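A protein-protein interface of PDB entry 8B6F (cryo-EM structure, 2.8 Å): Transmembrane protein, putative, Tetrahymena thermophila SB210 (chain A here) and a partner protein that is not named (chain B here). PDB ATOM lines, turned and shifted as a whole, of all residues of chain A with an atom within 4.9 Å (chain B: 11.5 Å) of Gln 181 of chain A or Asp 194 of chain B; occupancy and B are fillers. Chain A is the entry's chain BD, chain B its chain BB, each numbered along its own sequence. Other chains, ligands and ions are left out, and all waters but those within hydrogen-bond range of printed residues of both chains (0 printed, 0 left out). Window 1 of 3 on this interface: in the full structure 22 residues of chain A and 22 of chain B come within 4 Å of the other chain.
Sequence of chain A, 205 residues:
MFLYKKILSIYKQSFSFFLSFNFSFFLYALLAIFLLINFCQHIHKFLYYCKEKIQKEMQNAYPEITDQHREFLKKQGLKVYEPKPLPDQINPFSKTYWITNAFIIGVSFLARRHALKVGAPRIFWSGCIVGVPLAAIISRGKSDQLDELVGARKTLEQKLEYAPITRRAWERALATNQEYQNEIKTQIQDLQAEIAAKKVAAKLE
The side-chain amide nitrogen of Asn 195 of chain B sits close to the side-chain amide nitrogen of Asn 177 of chain A, 3.5 Å away.
The side-chain amide oxygen (OD1) of Asn 195 of chain B sits at hydrogen-bond distance from the side-chain amide nitrogen (NE2) of Gln 181 of chain A, 2.8 Å away.
The side-chain carboxylate (OD1) of Asp 194 of chain B sits at hydrogen-bond distance from the side-chain amide nitrogen (NE2) of Gln 190 of chain B (3.2 Å).
O of Ile 191 of chain B lies close to OD1 of Asn 195 of chain B (3.0 Å).
Among the printed residues, pairs that only touch across the chains: Asn 177 of chain A with Ile 191 of chain B (3.1 Å), Ile 184 of chain A with Leu 199 of chain B (3.6 Å), Ile 184 of chain A with Leu 198 of chain B (3.7 Å), Gln 181 of chain A with Leu 198 of chain B (3.9 Å), Gln 181 of chain A with Asp 194 of chain B (3.96 Å), Tyr 180 of chain A with Leu 199 of chain B (3.97 Å) and Lys 185 of chain A with Leu 198 of chain B (3.998 Å).
Of chain B, only Ile 191 (3.1 Å) and Asn 195 (3.5 Å) come within 4 Å of Asn 177 of chain A.
No residue of chain B comes within 4 Å of Gln 178 of chain A.
Of chain B, only Leu 199 comes within 4 Å of Tyr 180 of chain A.
Of chain B, only Asp 194, Asn 195 and Leu 198 come within 4 Å of Gln 181 of chain A.
No residue of chain B comes within 4 Å of Asn 182 of chain A.
Ile 184 of chain A touches just these residues of chain B: Leu 198 (3.7 Å) and Leu 199 (3.6 Å).
Of the printed residues of chain B, Lys 185 of chain A touches Leu 198.
Of the printed residues of chain A, Ile 191 of chain B touches Asn 177 (3.1 Å).
Asp 194 of chain B touches one residue of chain A.
Printed residues of chain A within 4 Å of Asn 195 of chain B: Asn 177 and Gln 181.
Printed residues of chain A within 4 Å of Leu 198 of chain B: Gln 181, Ile 184 and Lys 185.
The nearest printed residue of chain A that does not touch Leu 199 of chain B is Lys 185 of chain A (8.2 Å).
Of the 9 printed residues of chain A, 5 touch a printed residue of chain B.
Of the 19 printed residues of chain B, 5 touch a printed residue of chain A.
Hydrophobic or aromatic side chains of chain B within 4 Å of the printed part of chain A: Ile 191, Leu 198 and Leu 199.
Among the printed residues, 9 pairs touch across the chains.
Among the printed residues, no Asp or Glu carboxylate lies within 4 Å of a Lys or Arg side-chain nitrogen of the other chain.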
ATOM      1  N   ASN A 177     -23.382 -14.005 -28.523  1.00  0.00           N
ATOM      2  CA  ASN A 177     -24.296 -13.038 -27.929  1.00  0.00           C
ATOM      3  C   ASN A 177     -24.101 -11.660 -28.545  1.00  0.00           C
ATOM      4  O   ASN A 177     -25.075 -10.945 -28.803  1.00  0.00           O
ATOM      5  CB  ASN A 177     -24.085 -12.982 -26.418  1.00  0.00           C
ATOM      6  CG  ASN A 177     -24.899 -11.889 -25.758  1.00  0.00           C
ATOM      7  OD1 ASN A 177     -24.425 -11.218 -24.841  1.00  0.00           O
ATOM      8  ND2 ASN A 177     -26.134 -11.711 -26.209  1.00  0.00           N
ATOM      9  N   GLN A 178     -22.849 -11.271 -28.789  1.00  0.00           N
ATOM     10  CA  GLN A 178     -22.596  -9.981 -29.419  1.00  0.00           C
ATOM     11  C   GLN A 178     -23.188  -9.936 -30.820  1.00  0.00           C
ATOM     12  O   GLN A 178     -23.778  -8.927 -31.222  1.00  0.00           O
ATOM     13  CB  GLN A 178     -21.092  -9.708 -29.460  1.00  0.00           C
ATOM     14  CG  GLN A 178     -20.727  -8.296 -29.885  1.00  0.00           C
ATOM     15  CD  GLN A 178     -21.168  -7.253 -28.882  1.00  0.00           C
ATOM     16  OE1 GLN A 178     -21.630  -7.579 -27.789  1.00  0.00           O
ATOM     17  NE2 GLN A 178     -21.030  -5.984 -29.249  1.00  0.00           N
ATOM     18  N   GLU A 179     -23.035 -11.019 -31.586  1.00  0.00           N
ATOM     19  CA  GLU A 179     -23.640 -11.067 -32.914  1.00  0.00           C
ATOM     20  C   GLU A 179     -25.157 -10.979 -32.823  1.00  0.00           C
ATOM     21  O   GLU A 179     -25.797 -10.288 -33.623  1.00  0.00           O
ATOM     22  CB  GLU A 179     -23.222 -12.343 -33.646  1.00  0.00           C
ATOM     23  CG  GLU A 179     -21.919 -12.221 -34.428  1.00  0.00           C
ATOM     24  CD  GLU A 179     -20.715 -12.720 -33.653  1.00  0.00           C
ATOM     25  OE1 GLU A 179     -20.761 -13.864 -33.154  1.00  0.00           O
ATOM     26  OE2 GLU A 179     -19.720 -11.972 -33.544  1.00  0.00           O
ATOM     27  N   TYR A 180     -25.749 -11.679 -31.853  1.00  0.00           N
ATOM     28  CA  TYR A 180     -27.196 -11.630 -31.675  1.00  0.00           C
ATOM     29  C   TYR A 180     -27.664 -10.218 -31.346  1.00  0.00           C
ATOM     30  O   TYR A 180     -28.663  -9.742 -31.897  1.00  0.00           O
ATOM     31  CB  TYR A 180     -27.604 -12.607 -30.574  1.00  0.00           C
ATOM     32  CG  TYR A 180     -29.082 -12.640 -30.264  1.00  0.00           C
ATOM     33  CD1 TYR A 180     -29.968 -13.335 -31.079  1.00  0.00           C
ATOM     34  CD2 TYR A 180     -29.587 -12.008 -29.136  1.00  0.00           C
ATOM     35  CE1 TYR A 180     -31.318 -13.382 -30.789  1.00  0.00           C
ATOM     36  CE2 TYR A 180     -30.935 -12.048 -28.837  1.00  0.00           C
ATOM     37  CZ  TYR A 180     -31.795 -12.738 -29.667  1.00  0.00           C
ATOM     38  OH  TYR A 180     -33.138 -12.777 -29.374  1.00  0.00           O
ATOM     39  N   GLN A 181     -26.957  -9.534 -30.444  1.00  0.00           N
ATOM     40  CA  GLN A 181     -27.321  -8.164 -30.100  1.00  0.00           C
ATOM     41  C   GLN A 181     -27.174  -7.234 -31.297  1.00  0.00           C
ATOM     42  O   GLN A 181     -28.014  -6.355 -31.515  1.00  0.00           O
ATOM     43  CB  GLN A 181     -26.471  -7.674 -28.929  1.00  0.00           C
ATOM     44  CG  GLN A 181     -26.799  -8.359 -27.616  1.00  0.00           C
ATOM     45  CD  GLN A 181     -25.971  -7.834 -26.465  1.00  0.00           C
ATOM     46  OE1 GLN A 181     -25.019  -7.081 -26.663  1.00  0.00           O
ATOM     47  NE2 GLN A 181     -26.336  -8.225 -25.250  1.00  0.00           N
ATOM     48  N   ASN A 182     -26.112  -7.412 -32.084  1.00  0.00           N
ATOM     49  CA  ASN A 182     -25.937  -6.591 -33.277  1.00  0.00           C
ATOM     50  C   ASN A 182     -27.069  -6.816 -34.270  1.00  0.00           C
ATOM     51  O   ASN A 182     -27.563  -5.866 -34.887  1.00  0.00           O
ATOM     52  CB  ASN A 182     -24.589  -6.888 -33.933  1.00  0.00           C
ATOM     53  CG  ASN A 182     -23.420  -6.551 -33.033  1.00  0.00           C
ATOM     54  OD1 ASN A 182     -23.535  -5.723 -32.130  1.00  0.00           O
ATOM     55  ND2 ASN A 182     -22.281  -7.188 -33.281  1.00  0.00           N
ATOM     56  N   GLU A 183     -27.489  -8.069 -34.447  1.00  0.00           N
ATOM     57  CA  GLU A 183     -28.606  -8.342 -35.342  1.00  0.00           C
ATOM     58  C   GLU A 183     -29.882  -7.671 -34.853  1.00  0.00           C
ATOM     59  O   GLU A 183     -30.631  -7.092 -35.649  1.00  0.00           O
ATOM     60  CB  GLU A 183     -28.811  -9.851 -35.471  1.00  0.00           C
ATOM     61  CG  GLU A 183     -29.904 -10.246 -36.451  1.00  0.00           C
ATOM     62  CD  GLU A 183     -29.616  -9.780 -37.865  1.00  0.00           C
ATOM     63  OE1 GLU A 183     -28.435  -9.525 -38.179  1.00  0.00           O
ATOM     64  OE2 GLU A 183     -30.572  -9.662 -38.660  1.00  0.00           O
ATOM     65  N   ILE A 184     -30.153  -7.740 -33.549  1.00  0.00           N
ATOM     66  CA  ILE A 184     -31.351  -7.102 -33.009  1.00  0.00           C
ATOM     67  C   ILE A 184     -31.284  -5.592 -33.197  1.00  0.00           C
ATOM     68  O   ILE A 184     -32.285  -4.950 -33.535  1.00  0.00           O
ATOM     69  CB  ILE A 184     -31.546  -7.485 -31.530  1.00  0.00           C
ATOM     70  CG1 ILE A 184     -32.213  -8.859 -31.433  1.00  0.00           C
ATOM     71  CG2 ILE A 184     -32.382  -6.433 -30.805  1.00  0.00           C
ATOM     72  CD1 ILE A 184     -32.396  -9.370 -30.017  1.00  0.00           C
ATOM     73  N   LYS A 185     -30.107  -5.000 -32.980  1.00  0.00           N
ATOM     74  CA  LYS A 185     -29.968  -3.560 -33.166  1.00  0.00           C
ATOM     75  C   LYS A 185     -30.200  -3.166 -34.618  1.00  0.00           C
ATOM     76  O   LYS A 185     -30.849  -2.152 -34.897  1.00  0.00           O
ATOM     77  CB  LYS A 185     -28.586  -3.101 -32.700  1.00  0.00           C
ATOM     78  CG  LYS A 185     -28.392  -3.169 -31.193  1.00  0.00           C
ATOM     79  CD  LYS A 185     -26.990  -2.738 -30.792  1.00  0.00           C
ATOM     80  CE  LYS A 185     -26.811  -2.795 -29.284  1.00  0.00           C
ATOM     81  NZ  LYS A 185     -25.450  -2.357 -28.865  1.00  0.00           N
ATOM     82  N   GLU B 185     -22.081 -16.279 -13.552  1.00  0.00           N
ATOM     83  CA  GLU B 185     -23.527 -16.163 -13.398  1.00  0.00           C
ATOM     84  C   GLU B 185     -23.961 -14.704 -13.336  1.00  0.00           C
ATOM     85  O   GLU B 185     -24.979 -14.328 -13.925  1.00  0.00           O
ATOM     86  CB  GLU B 185     -23.986 -16.922 -12.155  1.00  0.00           C
ATOM     87  CG  GLU B 185     -23.916 -18.432 -12.318  1.00  0.00           C
ATOM     88  CD  GLU B 185     -24.509 -19.180 -11.142  1.00  0.00           C
ATOM     89  OE1 GLU B 185     -24.772 -18.545 -10.100  1.00  0.00           O
ATOM     90  OE2 GLU B 185     -24.716 -20.405 -11.263  1.00  0.00           O
ATOM     91  N   ASP B 186     -23.199 -13.862 -12.634  1.00  0.00           N
ATOM     92  CA  ASP B 186     -23.525 -12.440 -12.602  1.00  0.00           C
ATOM     93  C   ASP B 186     -23.465 -11.833 -13.997  1.00  0.00           C
ATOM     94  O   ASP B 186     -24.344 -11.055 -14.382  1.00  0.00           O
ATOM     95  CB  ASP B 186     -22.574 -11.702 -11.661  1.00  0.00           C
ATOM     96  CG  ASP B 186     -22.748 -12.115 -10.214  1.00  0.00           C
ATOM     97  OD1 ASP B 186     -23.886 -12.458  -9.827  1.00  0.00           O
ATOM     98  OD2 ASP B 186     -21.750 -12.096  -9.463  1.00  0.00           O
ATOM     99  N   LYS B 187     -22.433 -12.173 -14.771  1.00  0.00           N
ATOM    100  CA  LYS B 187     -22.339 -11.666 -16.135  1.00  0.00           C
ATOM    101  C   LYS B 187     -23.508 -12.157 -16.981  1.00  0.00           C
ATOM    102  O   LYS B 187     -24.019 -11.422 -17.833  1.00  0.00           O
ATOM    103  CB  LYS B 187     -21.008 -12.077 -16.760  1.00  0.00           C
ATOM    104  CG  LYS B 187     -19.812 -11.352 -16.165  1.00  0.00           C
ATOM    105  CD  LYS B 187     -18.549 -11.612 -16.966  1.00  0.00           C
ATOM    106  CE  LYS B 187     -17.355 -10.883 -16.369  1.00  0.00           C
ATOM    107  NZ  LYS B 187     -17.543  -9.406 -16.352  1.00  0.00           N
ATOM    108  N   ILE B 188     -23.943 -13.398 -16.763  1.00  0.00           N
ATOM    109  CA  ILE B 188     -25.093 -13.920 -17.495  1.00  0.00           C
ATOM    110  C   ILE B 188     -26.350 -13.139 -17.132  1.00  0.00           C
ATOM    111  O   ILE B 188     -27.193 -12.861 -17.991  1.00  0.00           O
ATOM    112  CB  ILE B 188     -25.261 -15.428 -17.233  1.00  0.00           C
ATOM    113  CG1 ILE B 188     -24.142 -16.208 -17.926  1.00  0.00           C
ATOM    114  CG2 ILE B 188     -26.621 -15.916 -17.730  1.00  0.00           C
ATOM    115  CD1 ILE B 188     -24.085 -17.674 -17.549  1.00  0.00           C
ATOM    116  N   ARG B 189     -26.502 -12.779 -15.854  1.00  0.00           N
ATOM    117  CA  ARG B 189     -27.643 -11.957 -15.464  1.00  0.00           C
ATOM    118  C   ARG B 189     -27.617 -10.614 -16.180  1.00  0.00           C
ATOM    119  O   ARG B 189     -28.650 -10.142 -16.667  1.00  0.00           O
ATOM    120  CB  ARG B 189     -27.652 -11.745 -13.951  1.00  0.00           C
ATOM    121  CG  ARG B 189     -27.889 -13.004 -13.142  1.00  0.00           C
ATOM    122  CD  ARG B 189     -28.041 -12.677 -11.664  1.00  0.00           C
ATOM    123  NE  ARG B 189     -28.075 -13.880 -10.842  1.00  0.00           N
ATOM    124  CZ  ARG B 189     -27.016 -14.432 -10.263  1.00  0.00           C
ATOM    125  NH1 ARG B 189     -25.808 -13.908 -10.387  1.00  0.00           N
ATOM    126  NH2 ARG B 189     -27.173 -15.537  -9.541  1.00  0.00           N
ATOM    127  N   GLN B 190     -26.447  -9.978 -16.247  1.00  0.00           N
ATOM    128  CA  GLN B 190     -26.348  -8.699 -16.940  1.00  0.00           C
ATOM    129  C   GLN B 190     -26.684  -8.852 -18.417  1.00  0.00           C
ATOM    130  O   GLN B 190     -27.376  -8.005 -18.996  1.00  0.00           O
ATOM    131  CB  GLN B 190     -24.946  -8.117 -16.764  1.00  0.00           C
ATOM    132  CG  GLN B 190     -24.768  -6.740 -17.381  1.00  0.00           C
ATOM    133  CD  GLN B 190     -25.703  -5.708 -16.783  1.00  0.00           C
ATOM    134  OE1 GLN B 190     -26.242  -5.899 -15.694  1.00  0.00           O
ATOM    135  NE2 GLN B 190     -25.901  -4.606 -17.496  1.00  0.00           N
ATOM    136  N   ILE B 191     -26.204  -9.927 -19.045  1.00  0.00           N
ATOM    137  CA  ILE B 191     -26.506 -10.167 -20.454  1.00  0.00           C
ATOM    138  C   ILE B 191     -28.000 -10.371 -20.648  1.00  0.00           C
ATOM    139  O   ILE B 191     -28.585  -9.894 -21.627  1.00  0.00           O
ATOM    140  CB  ILE B 191     -25.692 -11.366 -20.979  1.00  0.00           C
ATOM    141  CG1 ILE B 191     -24.207 -11.000 -21.053  1.00  0.00           C
ATOM    142  CG2 ILE B 191     -26.203 -11.804 -22.352  1.00  0.00           C
ATOM    143  CD1 ILE B 191     -23.296 -12.163 -21.388  1.00  0.00           C
ATOM    144  N   ARG B 192     -28.643 -11.093 -19.728  1.00  0.00           N
ATOM    145  CA  ARG B 192     -30.088 -11.265 -19.815  1.00  0.00           C
ATOM    146  C   ARG B 192     -30.806  -9.925 -19.743  1.00  0.00           C
ATOM    147  O   ARG B 192     -31.753  -9.678 -20.497  1.00  0.00           O
ATOM    148  CB  ARG B 192     -30.578 -12.181 -18.695  1.00  0.00           C
ATOM    149  CG  ARG B 192     -30.238 -13.645 -18.883  1.00  0.00           C
ATOM    150  CD  ARG B 192     -30.826 -14.480 -17.758  1.00  0.00           C
ATOM    151  NE  ARG B 192     -30.489 -15.891 -17.888  1.00  0.00           N
ATOM    152  CZ  ARG B 192     -30.827 -16.826 -17.013  1.00  0.00           C
ATOM    153  NH1 ARG B 192     -31.518 -16.537 -15.923  1.00  0.00           N
ATOM    154  NH2 ARG B 192     -30.461 -18.085 -17.236  1.00  0.00           N
ATOM    155  N   ILE B 193     -30.374  -9.049 -18.837  1.00  0.00           N
ATOM    156  CA  ILE B 193     -31.010  -7.740 -18.714  1.00  0.00           C
ATOM    157  C   ILE B 193     -30.861  -6.959 -20.015  1.00  0.00           C
ATOM    158  O   ILE B 193     -31.816  -6.344 -20.504  1.00  0.00           O
ATOM    159  CB  ILE B 193     -30.419  -6.973 -17.517  1.00  0.00           C
ATOM    160  CG1 ILE B 193     -30.803  -7.668 -16.208  1.00  0.00           C
ATOM    161  CG2 ILE B 193     -30.904  -5.530 -17.508  1.00  0.00           C
ATOM    162  CD1 ILE B 193     -30.089  -7.125 -14.985  1.00  0.00           C
ATOM    163  N   ASP B 194     -29.656  -6.966 -20.591  1.00  0.00           N
ATOM    164  CA  ASP B 194     -29.432  -6.231 -21.833  1.00  0.00           C
ATOM    165  C   ASP B 194     -30.282  -6.789 -22.966  1.00  0.00           C
ATOM    166  O   ASP B 194     -30.886  -6.030 -23.731  1.00  0.00           O
ATOM    167  CB  ASP B 194     -27.952  -6.274 -22.209  1.00  0.00           C
ATOM    168  CG  ASP B 194     -27.065  -5.652 -21.151  1.00  0.00           C
ATOM    169  OD1 ASP B 194     -27.598  -5.224 -20.106  1.00  0.00           O
ATOM    170  OD2 ASP B 194     -25.837  -5.587 -21.367  1.00  0.00           O
ATOM    171  N   ASN B 195     -30.333  -8.115 -23.095  1.00  0.00           N
ATOM    172  CA  ASN B 195     -31.139  -8.719 -24.148  1.00  0.00           C
ATOM    173  C   ASN B 195     -32.612  -8.392 -23.963  1.00  0.00           C
ATOM    174  O   ASN B 195     -33.323  -8.120 -24.936  1.00  0.00           O
ATOM    175  CB  ASN B 195     -30.928 -10.234 -24.169  1.00  0.00           C
ATOM    176  CG  ASN B 195     -29.509 -10.618 -24.533  1.00  0.00           C
ATOM    177  OD1 ASN B 195     -28.621  -9.769 -24.601  1.00  0.00           O
ATOM    178  ND2 ASN B 195     -29.288 -11.907 -24.766  1.00  0.00           N
ATOM    179  N   ASP B 196     -33.091  -8.417 -22.718  1.00  0.00           N
ATOM    180  CA  ASP B 196     -34.482  -8.066 -22.456  1.00  0.00           C
ATOM    181  C   ASP B 196     -34.764  -6.618 -22.827  1.00  0.00           C
ATOM    182  O   ASP B 196     -35.816  -6.313 -23.401  1.00  0.00           O
ATOM    183  CB  ASP B 196     -34.819  -8.317 -20.987  1.00  0.00           C
ATOM    184  CG  ASP B 196     -36.286  -8.090 -20.683  1.00  0.00           C
ATOM    185  OD1 ASP B 196     -37.114  -8.942 -21.068  1.00  0.00           O
ATOM    186  OD2 ASP B 196     -36.614  -7.058 -20.060  1.00  0.00           O
ATOM    187  N   LYS B 197     -33.839  -5.708 -22.514  1.00  0.00           N
ATOM    188  CA  LYS B 197     -34.034  -4.311 -22.889  1.00  0.00           C
ATOM    189  C   LYS B 197     -34.145  -4.163 -24.400  1.00  0.00           C
ATOM    190  O   LYS B 197     -35.028  -3.462 -24.904  1.00  0.00           O
ATOM    191  CB  LYS B 197     -32.886  -3.456 -22.351  1.00  0.00           C
ATOM    192  CG  LYS B 197     -32.995  -3.131 -20.868  1.00  0.00           C
ATOM    193  CD  LYS B 197     -31.916  -2.149 -20.440  1.00  0.00           C
ATOM    194  CE  LYS B 197     -32.161  -1.633 -19.030  1.00  0.00           C
ATOM    195  NZ  LYS B 197     -32.122  -2.716 -18.013  1.00  0.00           N
ATOM    196  N   LEU B 198     -33.250  -4.816 -25.141  1.00  0.00           N
ATOM    197  CA  LEU B 198     -33.298  -4.723 -26.596  1.00  0.00           C
ATOM    198  C   LEU B 198     -34.595  -5.305 -27.143  1.00  0.00           C
ATOM    199  O   LEU B 198     -35.214  -4.725 -28.043  1.00  0.00           O
ATOM    200  CB  LEU B 198     -32.090  -5.431 -27.204  1.00  0.00           C
ATOM    201  CG  LEU B 198     -30.884  -4.538 -27.502  1.00  0.00           C
ATOM    202  CD1 LEU B 198     -30.397  -3.842 -26.242  1.00  0.00           C
ATOM    203  CD2 LEU B 198     -29.765  -5.347 -28.135  1.00  0.00           C
ATOM    204  N   LEU B 199     -35.022  -6.453 -26.614  1.00  0.00           N
ATOM    205  CA  LEU B 199     -36.262  -7.065 -27.084  1.00  0.00           C
ATOM    206  C   LEU B 199     -37.463  -6.178 -26.787  1.00  0.00           C
ATOM    207  O   LEU B 199     -38.371  -6.052 -27.617  1.00  0.00           O
ATOM    208  CB  LEU B 199     -36.443  -8.444 -26.449  1.00  0.00           C
ATOM    209  CG  LEU B 199     -35.459  -9.529 -26.892  1.00  0.00           C
ATOM    210  CD1 LEU B 199     -35.675 -10.798 -26.088  1.00  0.00           C
ATOM    211  CD2 LEU B 199     -35.593  -9.815 -28.379  1.00  0.00           C
ATOM    212  N   GLN B 200     -37.490  -5.559 -25.606  1.00  0.00           N
ATOM    213  CA  GLN B 200     -38.588  -4.657 -25.278  1.00  0.00           C
ATOM    214  C   GLN B 200     -38.607  -3.455 -26.213  1.00  0.00           C
ATOM    215  O   GLN B 200     -39.678  -3.012 -26.644  1.00  0.00           O
ATOM    216  CB  GLN B 200     -38.484  -4.205 -23.821  1.00  0.00           C
ATOM    217  CG  GLN B 200     -38.739  -5.315 -22.809  1.00  0.00           C
ATOM    218  CD  GLN B 200     -40.144  -5.876 -22.897  1.00  0.00           C
ATOM    219  OE1 GLN B 200     -41.013  -5.308 -23.558  1.00  0.00           O
ATOM    220  NE2 GLN B 200     -40.374  -7.000 -22.229  1.00  0.00           N
ATOM    221  N   ARG B 201     -37.433  -2.910 -26.537  1.00  0.00           N
ATOM    222  CA  ARG B 201     -37.381  -1.800 -27.481  1.00  0.00           C
ATOM    223  C   ARG B 201     -37.912  -2.217 -28.846  1.00  0.00           C
ATOM    224  O   ARG B 201     -38.667  -1.472 -29.482  1.00  0.00           O
ATOM    225  CB  ARG B 201     -35.948  -1.279 -27.596  1.00  0.00           C
ATOM    226  CG  ARG B 201     -35.770  -0.135 -28.583  1.00  0.00           C
ATOM    227  CD  ARG B 201     -36.636   1.061 -28.219  1.00  0.00           C
ATOM    228  NE  ARG B 201     -36.418   2.189 -29.115  1.00  0.00           N
ATOM    229  CZ  ARG B 201     -37.061   3.346 -29.032  1.00  0.00           C
ATOM    230  NH1 ARG B 201     -37.975   3.564 -28.101  1.00  0.00           N
ATOM    231  NH2 ARG B 201     -36.781   4.308 -29.907  1.00  0.00           N
ATOM    232  N   LYS B 202     -37.527  -3.405 -29.317  1.00  0.00           N
ATOM    233  CA  LYS B 202     -38.017  -3.881 -30.606  1.00  0.00           C
ATOM    234  C   LYS B 202     -39.528  -4.061 -30.582  1.00  0.00           C
ATOM    235  O   LYS B 202     -40.219  -3.711 -31.546  1.00  0.00           O
ATOM    236  CB  LYS B 202     -37.327  -5.190 -30.982  1.00  0.00           C
ATOM    237  CG  LYS B 202     -37.680  -5.698 -32.371  1.00  0.00           C
ATOM    238  CD  LYS B 202     -36.898  -6.958 -32.710  1.00  0.00           C
ATOM    239  CE  LYS B 202     -37.160  -7.409 -34.138  1.00  0.00           C
ATOM    240  NZ  LYS B 202     -38.595  -7.719 -34.379  1.00  0.00           N
ATOM    241  N   ALA B 203     -40.059  -4.610 -29.488  1.00  0.00           N
ATOM    242  CA  ALA B 203     -41.503  -4.793 -29.376  1.00  0.00           C
ATOM    243  C   ALA B 203     -42.230  -3.455 -29.369  1.00  0.00           C
ATOM    244  O   ALA B 203     -43.287  -3.311 -29.994  1.00  0.00           O
ATOM    245  CB  ALA B 203     -41.834  -5.587 -28.112  1.00  0.00           C
